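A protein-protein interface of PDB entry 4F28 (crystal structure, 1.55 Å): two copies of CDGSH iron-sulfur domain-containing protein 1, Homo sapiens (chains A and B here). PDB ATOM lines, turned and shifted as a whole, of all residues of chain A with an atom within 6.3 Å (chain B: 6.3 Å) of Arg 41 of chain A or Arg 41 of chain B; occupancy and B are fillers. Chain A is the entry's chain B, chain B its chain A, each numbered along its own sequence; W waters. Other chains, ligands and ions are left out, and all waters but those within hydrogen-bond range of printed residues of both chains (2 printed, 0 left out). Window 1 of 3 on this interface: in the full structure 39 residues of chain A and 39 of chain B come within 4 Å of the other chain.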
ATOM      1  N   ILE A  13     -21.455 -33.989   7.143  1.00  0.00           N
ATOM      2  CA  ILE A  13     -21.866 -33.792   8.535  1.00  0.00           C
ATOM      3  C   ILE A  13     -22.791 -34.941   8.900  1.00  0.00           C
ATOM      4  O   ILE A  13     -22.571 -35.618   9.896  1.00  0.00           O
ATOM      5  CB  ILE A  13     -22.491 -32.391   8.710  1.00  0.00           C
ATOM      6  CG1 ILE A  13     -21.398 -31.319   8.669  1.00  0.00           C
ATOM      7  CG2 ILE A  13     -23.329 -32.279   9.977  1.00  0.00           C
ATOM      8  CD1 ILE A  13     -21.925 -29.938   8.316  1.00  0.00           C
ATOM      9  N   ILE A  24     -32.727 -32.541   4.338  1.00  0.00           N
ATOM     10  CA  ILE A  24     -33.504 -32.840   5.532  1.00  0.00           C
ATOM     11  C   ILE A  24     -33.860 -31.560   6.292  1.00  0.00           C
ATOM     12  O   ILE A  24     -32.989 -30.907   6.906  1.00  0.00           O
ATOM     13  CB  ILE A  24     -32.799 -33.866   6.431  1.00  0.00           C
ATOM     14  CG1 ILE A  24     -32.599 -35.181   5.668  1.00  0.00           C
ATOM     15  CG2 ILE A  24     -33.597 -34.125   7.727  1.00  0.00           C
ATOM     16  CD1 ILE A  24     -31.506 -36.093   6.346  1.00  0.00           C
ATOM     17  N   VAL A  25     -35.169 -31.252   6.275  1.00  0.00           N
ATOM     18  CA  VAL A  25     -35.760 -30.092   6.961  1.00  0.00           C
ATOM     19  C   VAL A  25     -36.862 -30.599   7.887  1.00  0.00           C
ATOM     20  O   VAL A  25     -37.652 -31.473   7.483  1.00  0.00           O
ATOM     21  CB  VAL A  25     -36.318 -29.030   5.944  1.00  0.00           C
ATOM     22  CG1 VAL A  25     -36.818 -27.781   6.657  1.00  0.00           C
ATOM     23  CG2 VAL A  25     -35.287 -28.651   4.889  1.00  0.00           C
ATOM     24  N   HIS A  26     -36.914 -30.059   9.116  1.00  0.00           N
ATOM     25  CA  HIS A  26     -37.996 -30.391  10.037  1.00  0.00           C
ATOM     26  C   HIS A  26     -38.728 -29.115  10.359  1.00  0.00           C
ATOM     27  O   HIS A  26     -38.080 -28.089  10.582  1.00  0.00           O
ATOM     28  CB  HIS A  26     -37.477 -31.070  11.327  1.00  0.00           C
ATOM     29  CG  HIS A  26     -37.037 -32.493  11.102  1.00  0.00           C
ATOM     30  ND1 HIS A  26     -35.767 -32.784  10.674  1.00  0.00           N
ATOM     31  CD2 HIS A  26     -37.740 -33.651  11.205  1.00  0.00           C
ATOM     32  CE1 HIS A  26     -35.719 -34.108  10.550  1.00  0.00           C
ATOM     33  NE2 HIS A  26     -36.891 -34.667  10.852  1.00  0.00           N
ATOM     34  N   TYR A  39     -33.507 -30.285  20.396  1.00  0.00           N
ATOM     35  CA  TYR A  39     -33.258 -30.662  19.010  1.00  0.00           C
ATOM     36  C   TYR A  39     -31.786 -30.917  18.703  1.00  0.00           C
ATOM     37  O   TYR A  39     -30.906 -30.139  19.059  1.00  0.00           O
ATOM     38  CB  TYR A  39     -33.824 -29.594  18.080  1.00  0.00           C
ATOM     39  CG  TYR A  39     -35.330 -29.462  18.189  1.00  0.00           C
ATOM     40  CD1 TYR A  39     -36.176 -30.343  17.517  1.00  0.00           C
ATOM     41  CD2 TYR A  39     -35.909 -28.414  18.900  1.00  0.00           C
ATOM     42  CE1 TYR A  39     -37.558 -30.215  17.594  1.00  0.00           C
ATOM     43  CE2 TYR A  39     -37.290 -28.268  18.975  1.00  0.00           C
ATOM     44  CZ  TYR A  39     -38.112 -29.181  18.329  1.00  0.00           C
ATOM     45  OH  TYR A  39     -39.473 -29.024  18.383  1.00  0.00           O
ATOM     46  N   CYS A  40     -31.537 -32.015  18.000  1.00  0.00           N
ATOM     47  CA  CYS A  40     -30.191 -32.406  17.628  1.00  0.00           C
ATOM     48  C   CYS A  40     -29.620 -31.511  16.490  1.00  0.00           C
ATOM     49  O   CYS A  40     -30.271 -31.266  15.458  1.00  0.00           O
ATOM     50  CB  CYS A  40     -30.187 -33.888  17.240  1.00  0.00           C
ATOM     51  SG  CYS A  40     -28.590 -34.500  16.660  1.00  0.00           S
ATOM     52  N   ARG A  41     -28.382 -31.046  16.685  1.00  0.00           N
ATOM     53  CA  ARG A  41     -27.673 -30.284  15.666  1.00  0.00           C
ATOM     54  C   ARG A  41     -26.390 -31.029  15.216  1.00  0.00           C
ATOM     55  O   ARG A  41     -25.588 -30.453  14.495  1.00  0.00           O
ATOM     56  CB  ARG A  41     -27.333 -28.862  16.169  1.00  0.00           C
ATOM     57  CG  ARG A  41     -28.577 -28.017  16.460  1.00  0.00           C
ATOM     58  CD  ARG A  41     -28.298 -26.541  16.644  1.00  0.00           C
ATOM     59  NE  ARG A  41     -27.500 -26.315  17.856  1.00  0.00           N
ATOM     60  CZ  ARG A  41     -27.295 -25.118  18.392  1.00  0.00           C
ATOM     61  NH1 ARG A  41     -27.845 -24.037  17.854  1.00  0.00           N
ATOM     62  NH2 ARG A  41     -26.520 -24.987  19.459  1.00  0.00           N
ATOM     63  N   CYS A  42     -26.200 -32.299  15.645  1.00  0.00           N
ATOM     64  CA  CYS A  42     -24.976 -33.058  15.344  1.00  0.00           C
ATOM     65  C   CYS A  42     -25.227 -34.203  14.380  1.00  0.00           C
ATOM     66  O   CYS A  42     -24.252 -34.818  13.964  1.00  0.00           O
ATOM     67  CB  CYS A  42     -24.299 -33.579  16.621  1.00  0.00           C
ATOM     68  SG  CYS A  42     -25.174 -34.948  17.433  1.00  0.00           S
ATOM     69  N   TRP A  43     -26.496 -34.550  14.084  1.00  0.00           N
ATOM     70  CA  TRP A  43     -26.810 -35.620  13.130  1.00  0.00           C
ATOM     71  C   TRP A  43     -26.232 -37.001  13.567  1.00  0.00           C
ATOM     72  O   TRP A  43     -25.949 -37.852  12.709  1.00  0.00           O
ATOM     73  CB  TRP A  43     -26.337 -35.225  11.701  1.00  0.00           C
ATOM     74  CG  TRP A  43     -26.917 -33.912  11.238  1.00  0.00           C
ATOM     75  CD1 TRP A  43     -26.474 -32.664  11.563  1.00  0.00           C
ATOM     76  CD2 TRP A  43     -28.108 -33.723  10.458  1.00  0.00           C
ATOM     77  NE1 TRP A  43     -27.286 -31.708  10.998  1.00  0.00           N
ATOM     78  CE2 TRP A  43     -28.307 -32.328  10.329  1.00  0.00           C
ATOM     79  CE3 TRP A  43     -29.015 -34.597   9.835  1.00  0.00           C
ATOM     80  CZ2 TRP A  43     -29.377 -31.776   9.610  1.00  0.00           C
ATOM     81  CZ3 TRP A  43     -30.080 -34.051   9.117  1.00  0.00           C
ATOM     82  CH2 TRP A  43     -30.247 -32.657   8.992  1.00  0.00           C
ATOM     83  N   ARG A  44     -26.104 -37.227  14.899  1.00  0.00           N
ATOM     84  CA  ARG A  44     -25.615 -38.484  15.469  1.00  0.00           C
ATOM     85  C   ARG A  44     -26.655 -39.122  16.382  1.00  0.00           C
ATOM     86  O   ARG A  44     -26.523 -40.303  16.745  1.00  0.00           O
ATOM     87  CB  ARG A  44     -24.289 -38.290  16.240  1.00  0.00           C
ATOM     88  CG  ARG A  44     -23.113 -37.772  15.413  1.00  0.00           C
ATOM     89  CD  ARG A  44     -22.639 -38.749  14.341  1.00  0.00           C
ATOM     90  NE  ARG A  44     -21.530 -38.163  13.597  1.00  0.00           N
ATOM     91  CZ  ARG A  44     -21.684 -37.416  12.512  1.00  0.00           C
ATOM     92  NH1 ARG A  44     -22.898 -37.187  12.023  1.00  0.00           N
ATOM     93  NH2 ARG A  44     -20.631 -36.874  11.921  1.00  0.00           N
ATOM     94  N   PHE A  48     -33.105 -38.667  16.089  1.00  0.00           N
ATOM     95  CA  PHE A  48     -33.157 -37.484  15.197  1.00  0.00           C
ATOM     96  C   PHE A  48     -34.610 -37.254  14.713  1.00  0.00           C
ATOM     97  O   PHE A  48     -35.286 -38.243  14.394  1.00  0.00           O
ATOM     98  CB  PHE A  48     -32.193 -37.623  13.997  1.00  0.00           C
ATOM     99  CG  PHE A  48     -31.841 -36.285  13.382  1.00  0.00           C
ATOM    100  CD1 PHE A  48     -30.858 -35.473  13.955  1.00  0.00           C
ATOM    101  CD2 PHE A  48     -32.551 -35.790  12.288  1.00  0.00           C
ATOM    102  CE1 PHE A  48     -30.570 -34.204  13.417  1.00  0.00           C
ATOM    103  CE2 PHE A  48     -32.278 -34.518  11.769  1.00  0.00           C
ATOM    104  CZ  PHE A  48     -31.303 -33.721  12.350  1.00  0.00           C
ATOM    105  N   PRO A  49     -35.161 -36.025  14.770  1.00  0.00           N
ATOM    106  CA  PRO A  49     -34.495 -34.722  15.024  1.00  0.00           C
ATOM    107  C   PRO A  49     -34.266 -34.328  16.494  1.00  0.00           C
ATOM    108  O   PRO A  49     -33.772 -33.209  16.750  1.00  0.00           O
ATOM    109  CB  PRO A  49     -35.467 -33.739  14.373  1.00  0.00           C
ATOM    110  CG  PRO A  49     -36.810 -34.363  14.623  1.00  0.00           C
ATOM    111  CD  PRO A  49     -36.565 -35.822  14.361  1.00  0.00           C
ATOM    112  N   CYS A  51     -32.450 -34.580  20.322  1.00  0.00           N
ATOM    113  CA  CYS A  51     -31.147 -34.829  20.931  1.00  0.00           C
ATOM    114  C   CYS A  51     -31.302 -35.992  21.920  1.00  0.00           C
ATOM    115  O   CYS A  51     -32.253 -36.014  22.714  1.00  0.00           O
ATOM    116  CB  CYS A  51     -30.660 -33.550  21.628  1.00  0.00           C
ATOM    117  SG  CYS A  51     -29.136 -33.710  22.591  1.00  0.00           S
ATOM    118  N   VAL A  66     -20.030 -29.145  19.462  1.00  0.00           N
ATOM    119  CA  VAL A  66     -21.409 -28.960  19.046  1.00  0.00           C
ATOM    120  C   VAL A  66     -22.369 -29.385  20.154  1.00  0.00           C
ATOM    121  O   VAL A  66     -22.028 -30.196  21.022  1.00  0.00           O
ATOM    122  CB  VAL A  66     -21.713 -29.682  17.696  1.00  0.00           C
ATOM    123  CG1 VAL A  66     -20.900 -29.050  16.579  1.00  0.00           C
ATOM    124  CG2 VAL A  66     -21.448 -31.177  17.768  1.00  0.00           C
ATOM    125  N   GLY A  67     -23.576 -28.834  20.088  1.00  0.00           N
ATOM    126  CA  GLY A  67     -24.619 -29.145  21.044  1.00  0.00           C
ATOM    127  C   GLY A  67     -25.987 -28.810  20.498  1.00  0.00           C
ATOM    128  O   GLY A  67     -26.095 -28.244  19.409  1.00  0.00           O
ATOM    129  N   PRO A  68     -27.042 -29.131  21.276  1.00  0.00           N
ATOM    130  CA  PRO A  68     -28.406 -28.978  20.766  1.00  0.00           C
ATOM    131  C   PRO A  68     -29.007 -27.573  20.878  1.00  0.00           C
ATOM    132  O   PRO A  68     -28.421 -26.632  21.438  1.00  0.00           O
ATOM    133  CB  PRO A  68     -29.191 -29.949  21.655  1.00  0.00           C
ATOM    134  CG  PRO A  68     -28.468 -29.865  22.984  1.00  0.00           C
ATOM    135  CD  PRO A  68     -27.037 -29.869  22.561  1.00  0.00           C
ATOM    136  N   LEU A  69     -30.222 -27.470  20.300  1.00  0.00           N
ATOM    137  CA  LEU A  69     -31.096 -26.305  20.344  1.00  0.00           C
ATOM    138  C   LEU A  69     -32.275 -26.654  21.259  1.00  0.00           C
ATOM    139  O   LEU A  69     -32.968 -27.662  21.038  1.00  0.00           O
ATOM    140  CB  LEU A  69     -31.573 -25.934  18.944  1.00  0.00           C
ATOM    141  CG  LEU A  69     -32.605 -24.792  18.872  1.00  0.00           C
ATOM    142  CD1 LEU A  69     -31.926 -23.417  18.989  1.00  0.00           C
ATOM    143  CD2 LEU A  69     -33.420 -24.879  17.649  1.00  0.00           C
ATOM    144  N   ILE B  13     -17.749 -31.541  12.997  1.00  0.00           N
ATOM    145  CA  ILE B  13     -18.930 -31.029  12.307  1.00  0.00           C
ATOM    146  C   ILE B  13     -18.810 -29.510  12.268  1.00  0.00           C
ATOM    147  O   ILE B  13     -18.943 -28.897  11.205  1.00  0.00           O
ATOM    148  CB  ILE B  13     -20.204 -31.528  13.032  1.00  0.00           C
ATOM    149  CG1 ILE B  13     -20.394 -33.036  12.773  1.00  0.00           C
ATOM    150  CG2 ILE B  13     -21.440 -30.671  12.680  1.00  0.00           C
ATOM    151  CD1 ILE B  13     -21.272 -33.764  13.735  1.00  0.00           C
ATOM    152  N   ILE B  24     -21.491 -25.788  22.350  1.00  0.00           N
ATOM    153  CA  ILE B  24     -22.417 -24.759  21.897  1.00  0.00           C
ATOM    154  C   ILE B  24     -23.871 -25.257  21.962  1.00  0.00           C
ATOM    155  O   ILE B  24     -24.296 -26.113  21.177  1.00  0.00           O
ATOM    156  CB  ILE B  24     -22.061 -24.237  20.485  1.00  0.00           C
ATOM    157  CG1 ILE B  24     -20.639 -23.625  20.485  1.00  0.00           C
ATOM    158  CG2 ILE B  24     -23.091 -23.179  20.024  1.00  0.00           C
ATOM    159  CD1 ILE B  24     -20.061 -23.511  19.048  1.00  0.00           C
ATOM    160  N   VAL B  25     -24.617 -24.656  22.904  1.00  0.00           N
ATOM    161  CA  VAL B  25     -26.033 -24.917  23.168  1.00  0.00           C
ATOM    162  C   VAL B  25     -26.782 -23.592  23.068  1.00  0.00           C
ATOM    163  O   VAL B  25     -26.315 -22.575  23.596  1.00  0.00           O
ATOM    164  CB  VAL B  25     -26.271 -25.579  24.566  1.00  0.00           C
ATOM    165  CG1 VAL B  25     -27.735 -26.015  24.727  1.00  0.00           C
ATOM    166  CG2 VAL B  25     -25.349 -26.773  24.798  1.00  0.00           C
ATOM    167  N   HIS B  26     -27.954 -23.593  22.423  1.00  0.00           N
ATOM    168  CA  HIS B  26     -28.807 -22.406  22.396  1.00  0.00           C
ATOM    169  C   HIS B  26     -30.136 -22.797  23.022  1.00  0.00           C
ATOM    170  O   HIS B  26     -30.622 -23.903  22.787  1.00  0.00           O
ATOM    171  CB  HIS B  26     -28.997 -21.830  20.991  1.00  0.00           C
ATOM    172  CG  HIS B  26     -27.771 -21.176  20.451  1.00  0.00           C
ATOM    173  ND1 HIS B  26     -26.772 -21.915  19.824  1.00  0.00           N
ATOM    174  CD2 HIS B  26     -27.410 -19.872  20.471  1.00  0.00           C
ATOM    175  CE1 HIS B  26     -25.831 -21.033  19.501  1.00  0.00           C
ATOM    176  NE2 HIS B  26     -26.168 -19.794  19.880  1.00  0.00           N
ATOM    177  N   TYR B  39     -33.661 -22.384  12.198  1.00  0.00           N
ATOM    178  CA  TYR B  39     -32.415 -22.670  12.905  1.00  0.00           C
ATOM    179  C   TYR B  39     -31.434 -23.511  12.086  1.00  0.00           C
ATOM    180  O   TYR B  39     -31.809 -24.503  11.462  1.00  0.00           O
ATOM    181  CB  TYR B  39     -32.745 -23.350  14.234  1.00  0.00           C
ATOM    182  CG  TYR B  39     -33.524 -22.452  15.170  1.00  0.00           C
ATOM    183  CD1 TYR B  39     -32.874 -21.516  15.971  1.00  0.00           C
ATOM    184  CD2 TYR B  39     -34.895 -22.621  15.350  1.00  0.00           C
ATOM    185  CE1 TYR B  39     -33.586 -20.693  16.846  1.00  0.00           C
ATOM    186  CE2 TYR B  39     -35.611 -21.832  16.249  1.00  0.00           C
ATOM    187  CZ  TYR B  39     -34.956 -20.851  16.976  1.00  0.00           C
ATOM    188  OH  TYR B  39     -35.638 -20.057  17.872  1.00  0.00           O
ATOM    189  N   CYS B  40     -30.178 -23.097  12.080  1.00  0.00           N
ATOM    190  CA  CYS B  40     -29.110 -23.771  11.348  1.00  0.00           C
ATOM    191  C   CYS B  40     -28.722 -25.103  12.033  1.00  0.00           C
ATOM    192  O   CYS B  40     -28.494 -25.158  13.249  1.00  0.00           O
ATOM    193  CB  CYS B  40     -27.894 -22.847  11.218  1.00  0.00           C
ATOM    194  SG  CYS B  40     -26.447 -23.619  10.450  1.00  0.00           S
ATOM    195  N   ARG B  41     -28.615 -26.163  11.238  1.00  0.00           N
ATOM    196  CA  ARG B  41     -28.167 -27.471  11.736  1.00  0.00           C
ATOM    197  C   ARG B  41     -26.876 -27.922  11.014  1.00  0.00           C
ATOM    198  O   ARG B  41     -26.470 -29.078  11.151  1.00  0.00           O
ATOM    199  CB  ARG B  41     -29.274 -28.527  11.569  1.00  0.00           C
ATOM    200  CG  ARG B  41     -30.511 -28.235  12.428  1.00  0.00           C
ATOM    201  CD  ARG B  41     -31.440 -29.432  12.478  1.00  0.00           C
ATOM    202  NE  ARG B  41     -32.053 -29.732  11.176  1.00  0.00           N
ATOM    203  CZ  ARG B  41     -33.066 -30.570  11.032  1.00  0.00           C
ATOM    204  NH1 ARG B  41     -33.609 -31.154  12.095  1.00  0.00           N
ATOM    205  NH2 ARG B  41     -33.549 -30.835   9.823  1.00  0.00           N
ATOM    206  N   CYS B  42     -26.239 -27.016  10.244  1.00  0.00           N
ATOM    207  CA  CYS B  42     -25.048 -27.373   9.458  1.00  0.00           C
ATOM    208  C   CYS B  42     -23.784 -26.724   9.991  1.00  0.00           C
ATOM    209  O   CYS B  42     -22.705 -27.071   9.513  1.00  0.00           O
ATOM    210  CB  CYS B  42     -25.239 -27.055   7.973  1.00  0.00           C
ATOM    211  SG  CYS B  42     -25.181 -25.284   7.548  1.00  0.00           S
ATOM    212  N   TRP B  43     -23.909 -25.764  10.922  1.00  0.00           N
ATOM    213  CA  TRP B  43     -22.740 -25.096  11.528  1.00  0.00           C
ATOM    214  C   TRP B  43     -21.863 -24.382  10.463  1.00  0.00           C
ATOM    215  O   TRP B  43     -20.643 -24.255  10.637  1.00  0.00           O
ATOM    216  CB  TRP B  43     -21.916 -26.125  12.348  1.00  0.00           C
ATOM    217  CG  TRP B  43     -22.718 -26.802  13.417  1.00  0.00           C
ATOM    218  CD1 TRP B  43     -23.563 -27.859  13.262  1.00  0.00           C
ATOM    219  CD2 TRP B  43     -22.857 -26.371  14.774  1.00  0.00           C
ATOM    220  NE1 TRP B  43     -24.164 -28.162  14.458  1.00  0.00           N
ATOM    221  CE2 TRP B  43     -23.760 -27.259  15.402  1.00  0.00           C
ATOM    222  CE3 TRP B  43     -22.248 -25.360  15.539  1.00  0.00           C
ATOM    223  CZ2 TRP B  43     -24.092 -27.154  16.754  1.00  0.00           C
ATOM    224  CZ3 TRP B  43     -22.577 -25.250  16.875  1.00  0.00           C
ATOM    225  CH2 TRP B  43     -23.463 -26.152  17.483  1.00  0.00           C
ATOM    226  N   ARG B  44     -22.494 -23.888   9.371  1.00  0.00           N
ATOM    227  CA  ARG B  44     -21.810 -23.148   8.305  1.00  0.00           C
ATOM    228  C   ARG B  44     -22.419 -21.755   8.155  1.00  0.00           C
ATOM    229  O   ARG B  44     -21.827 -20.911   7.496  1.00  0.00           O
ATOM    230  CB  ARG B  44     -21.831 -23.905   6.958  1.00  0.00           C
ATOM    231  CG  ARG B  44     -21.143 -25.267   6.973  1.00  0.00           C
ATOM    232  CD  ARG B  44     -19.631 -25.234   7.194  1.00  0.00           C
ATOM    233  NE  ARG B  44     -19.091 -26.601   7.199  1.00  0.00           N
ATOM    234  CZ  ARG B  44     -19.007 -27.377   8.277  1.00  0.00           C
ATOM    235  NH1 ARG B  44     -19.367 -26.914   9.468  1.00  0.00           N
ATOM    236  NH2 ARG B  44     -18.544 -28.620   8.172  1.00  0.00           N
ATOM    237  N   PHE B  48     -25.315 -17.969  12.659  1.00  0.00           N
ATOM    238  CA  PHE B  48     -25.539 -19.024  13.660  1.00  0.00           C
ATOM    239  C   PHE B  48     -26.020 -18.402  14.979  1.00  0.00           C
ATOM    240  O   PHE B  48     -25.481 -17.363  15.379  1.00  0.00           O
ATOM    241  CB  PHE B  48     -24.295 -19.915  13.858  1.00  0.00           C
ATOM    242  CG  PHE B  48     -24.639 -21.277  14.419  1.00  0.00           C
ATOM    243  CD1 PHE B  48     -25.082 -22.302  13.588  1.00  0.00           C
ATOM    244  CD2 PHE B  48     -24.589 -21.513  15.780  1.00  0.00           C
ATOM    245  CE1 PHE B  48     -25.435 -23.548  14.120  1.00  0.00           C
ATOM    246  CE2 PHE B  48     -24.965 -22.740  16.312  1.00  0.00           C
ATOM    247  CZ  PHE B  48     -25.396 -23.750  15.479  1.00  0.00           C
ATOM    248  N   PRO B  49     -27.100 -18.907  15.619  1.00  0.00           N
ATOM    249  CA  PRO B  49     -27.806 -20.188  15.376  1.00  0.00           C
ATOM    250  C   PRO B  49     -28.895 -20.177  14.291  1.00  0.00           C
ATOM    251  O   PRO B  49     -29.565 -21.206  14.099  1.00  0.00           O
ATOM    252  CB  PRO B  49     -28.440 -20.467  16.742  1.00  0.00           C
ATOM    253  CG  PRO B  49     -28.790 -19.071  17.249  1.00  0.00           C
ATOM    254  CD  PRO B  49     -27.578 -18.269  16.866  1.00  0.00           C
ATOM    255  N   CYS B  51     -30.386 -20.009  10.336  1.00  0.00           N
ATOM    256  CA  CYS B  51     -30.041 -20.468   9.002  1.00  0.00           C
ATOM    257  C   CYS B  51     -29.936 -19.263   8.060  1.00  0.00           C
ATOM    258  O   CYS B  51     -30.829 -18.414   8.085  1.00  0.00           O
ATOM    259  CB  CYS B  51     -31.110 -21.457   8.529  1.00  0.00           C
ATOM    260  SG  CYS B  51     -30.871 -22.111   6.847  1.00  0.00           S
ATOM    261  N   VAL B  66     -28.061 -32.076   4.518  1.00  0.00           N
ATOM    262  CA  VAL B  66     -28.503 -31.430   5.745  1.00  0.00           C
ATOM    263  C   VAL B  66     -29.302 -30.160   5.439  1.00  0.00           C
ATOM    264  O   VAL B  66     -29.150 -29.552   4.383  1.00  0.00           O
ATOM    265  CB  VAL B  66     -27.337 -31.153   6.724  1.00  0.00           C
ATOM    266  CG1 VAL B  66     -26.725 -32.455   7.204  1.00  0.00           C
ATOM    267  CG2 VAL B  66     -26.282 -30.265   6.086  1.00  0.00           C
ATOM    268  N   GLY B  67     -30.145 -29.780   6.382  1.00  0.00           N
ATOM    269  CA  GLY B  67     -30.993 -28.603   6.273  1.00  0.00           C
ATOM    270  C   GLY B  67     -31.471 -28.135   7.629  1.00  0.00           C
ATOM    271  O   GLY B  67     -31.205 -28.790   8.639  1.00  0.00           O
ATOM    272  N   PRO B  68     -32.216 -27.017   7.656  1.00  0.00           N
ATOM    273  CA  PRO B  68     -32.572 -26.405   8.949  1.00  0.00           C
ATOM    274  C   PRO B  68     -33.794 -26.992   9.674  1.00  0.00           C
ATOM    275  O   PRO B  68     -34.506 -27.859   9.176  1.00  0.00           O
ATOM    276  CB  PRO B  68     -32.859 -24.947   8.547  1.00  0.00           C
ATOM    277  CG  PRO B  68     -33.433 -25.074   7.139  1.00  0.00           C
ATOM    278  CD  PRO B  68     -32.528 -26.106   6.524  1.00  0.00           C
ATOM    279  N   LEU B  69     -33.998 -26.473  10.902  1.00  0.00           N
ATOM    280  CA  LEU B  69     -35.124 -26.753  11.786  1.00  0.00           C
ATOM    281  C   LEU B  69     -35.991 -25.509  11.814  1.00  0.00           C
ATOM    282  O   LEU B  69     -35.510 -24.411  12.137  1.00  0.00           O
ATOM    283  CB  LEU B  69     -34.634 -27.127  13.214  1.00  0.00           C
ATOM    284  CG  LEU B  69     -35.738 -27.321  14.260  1.00  0.00           C
ATOM    285  CD1 LEU B  69     -36.378 -28.693  14.162  1.00  0.00           C
ATOM    286  CD2 LEU B  69     -35.208 -27.111  15.622  1.00  0.00           C
HETATM  287  O   HOH W   1     -29.364 -23.650  15.474  1.00  0.00           O
HETATM  288  O   HOH W   2     -32.861 -31.214  14.845  1.00  0.00           O
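NH2 of Arg 41 of chain A lies within hydrogen-bond range of O of Ile 24 of chain B (3.0 Å).
The backbone carbonyl oxygen (O) of Ile 24 of chain B sits at hydrogen-bond distance from the backbone NH (N) of Gly 67 of chain A (3.0 Å).
The guanidinium group (NH1) of Arg 41 of chain A is in hydrogen-bond range of a ring nitrogen (ND1) of His 26 of chain B, 3.1 Å away.
The backbone carbonyl oxygen (O) of Pro 68 of chain A is in hydrogen-bond range of the backbone NH (N) of His 26 of chain B (3.2 Å).
The backbone carbonyl oxygen (O) of Ile 24 of chain A lies within hydrogen-bond range of the guanidinium group (NH2) of Arg 41 of chain B (3.0 Å).
The guanidinium group (NH1) of Arg 41 of chain B is in hydrogen-bond range of a ring nitrogen (ND1) of His 26 of chain A.
The backbone carbonyl oxygen (O) of Arg 41 of chain B lies within hydrogen-bond range of the indole nitrogen (NE1) of Trp 43 of chain A (2.8 Å).
The backbone carbonyl oxygen (O) of Arg 41 of chain A is in hydrogen-bond range of the indole nitrogen (NE1) of Trp 43 of chain B (2.7 Å).
The backbone carbonyl oxygen of Ile 24 of chain A sits at hydrogen-bond distance from the backbone NH of Gly 67 of chain B (3.1 Å).
O of Pro 68 of chain B sits at hydrogen-bond distance from N of His 26 of chain A, 3.3 Å away.
The backbone NH (N) of Tyr 39 of chain B lies within hydrogen-bond range of the backbone carbonyl oxygen (O) of Leu 69 of chain B, at 2.7 Å.
The backbone NH of Trp 43 of chain B lies close to the side-chain sulfur of Cys 40 of chain B (3.4 Å).
The guanidinium group (NE) of Arg 41 of chain B sits at hydrogen-bond distance from the backbone carbonyl oxygen (O) of Gly 67 of chain B (2.8 Å).
The backbone carbonyl oxygen of Ile 13 of chain A is in hydrogen-bond range of the guanidinium group of Arg 44 of chain A (2.7 Å).
The backbone NH (N) of Tyr 39 of chain A sits at hydrogen-bond distance from the backbone carbonyl oxygen (O) of Leu 69 of chain A.
The backbone carbonyl oxygen (O) of Gly 67 of chain A sits at hydrogen-bond distance from the guanidinium group (NE) of Arg 41 of chain A, 2.8 Å away.
Val 25 of chain A touches Pro 68 of chain B (CA to O, 3.4 Å).
CG of Tyr 39 of chain A touches CD2 of Leu 69 of chain B, 3.5 Å away.
NH1 of Arg 41 of chain A touches CZ of Phe 48 of chain B, at 3.4 Å.
Cys 42 of chain A touches Ile 13 of chain B.
Ile 13 of chain B touches Arg 44 of chain A (CD1 to NH2, 3.7 Å).
Ile 24 of chain B touches Val 66 of chain A (O to C, 3.9 Å).
Gly 67 of chain A touches Trp 43 of chain B.
Pro 68 of chain A touches Val 25 of chain B.
CD2 of Leu 69 of chain A touches CG of Tyr 39 of chain B (3.5 Å).
CD2 of Leu 69 of chain A touches CD2 of Leu 69 of chain B, 3.5 Å away.
Of the printed residues of chain B, Val 25 of chain A touches Arg 41 (3.7 Å) and Pro 68 (3.4 Å).
Cys 51 of chain A touches none of the printed residues of chain B.
Printed residues of chain B within 4 Å of Gly 67 of chain A: Ile 24 (3.0 Å) and Trp 43 (3.5 Å).
Printed residues of chain A within 4 Å of Val 25 of chain B: Arg 41 and Pro 68.
Arg 41 of chain B touches eight residues of chain A.
Cys 51 of chain B touches none of the printed residues of chain A.
The nearest printed residue of chain A that does not touch Val 66 of chain B is Ile 24 of chain A (4.04 Å).
Hydrophobic or aromatic side chains of chain A within 4 Å of the printed part of chain B: Ile 13, Ile 24, Val 25, His 26, Tyr 39, Trp 43, Phe 48, Pro 49, Val 66 and Leu 69.
Among the printed residues, 36 pairs touch across the chains.
Ile 13 of chain A touches Cys 42 of chain B, and with the chains exchanged Cys 42 of chain A touches Ile 13 of chain B.
Tyr 39 of chain A touches Leu 69 of chain B, and with the chains exchanged Leu 69 of chain A touches Tyr 39 of chain B.
Arg 41 of chain A touches Phe 48 of chain B, and with the chains exchanged Phe 48 of chain A touches Arg 41 of chain B.
Trp 43 of chain A touches Val 66 of chain B, and with the chains exchanged Val 66 of chain A touches Trp 43 of chain B.
17 positions are printed for both chains.
Water W2 lies within hydrogen-bond range of O of Cys 40 of chain A, NH1 of Arg 41 of chain B and O of Pro 49 of chain A.
Water W1 lies within hydrogen-bond range of O of Pro 49 of chain B (2.8 Å), O of Cys 40 of chain B (2.8 Å) and NH1 of Arg 41 of chain A (2.8 Å).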
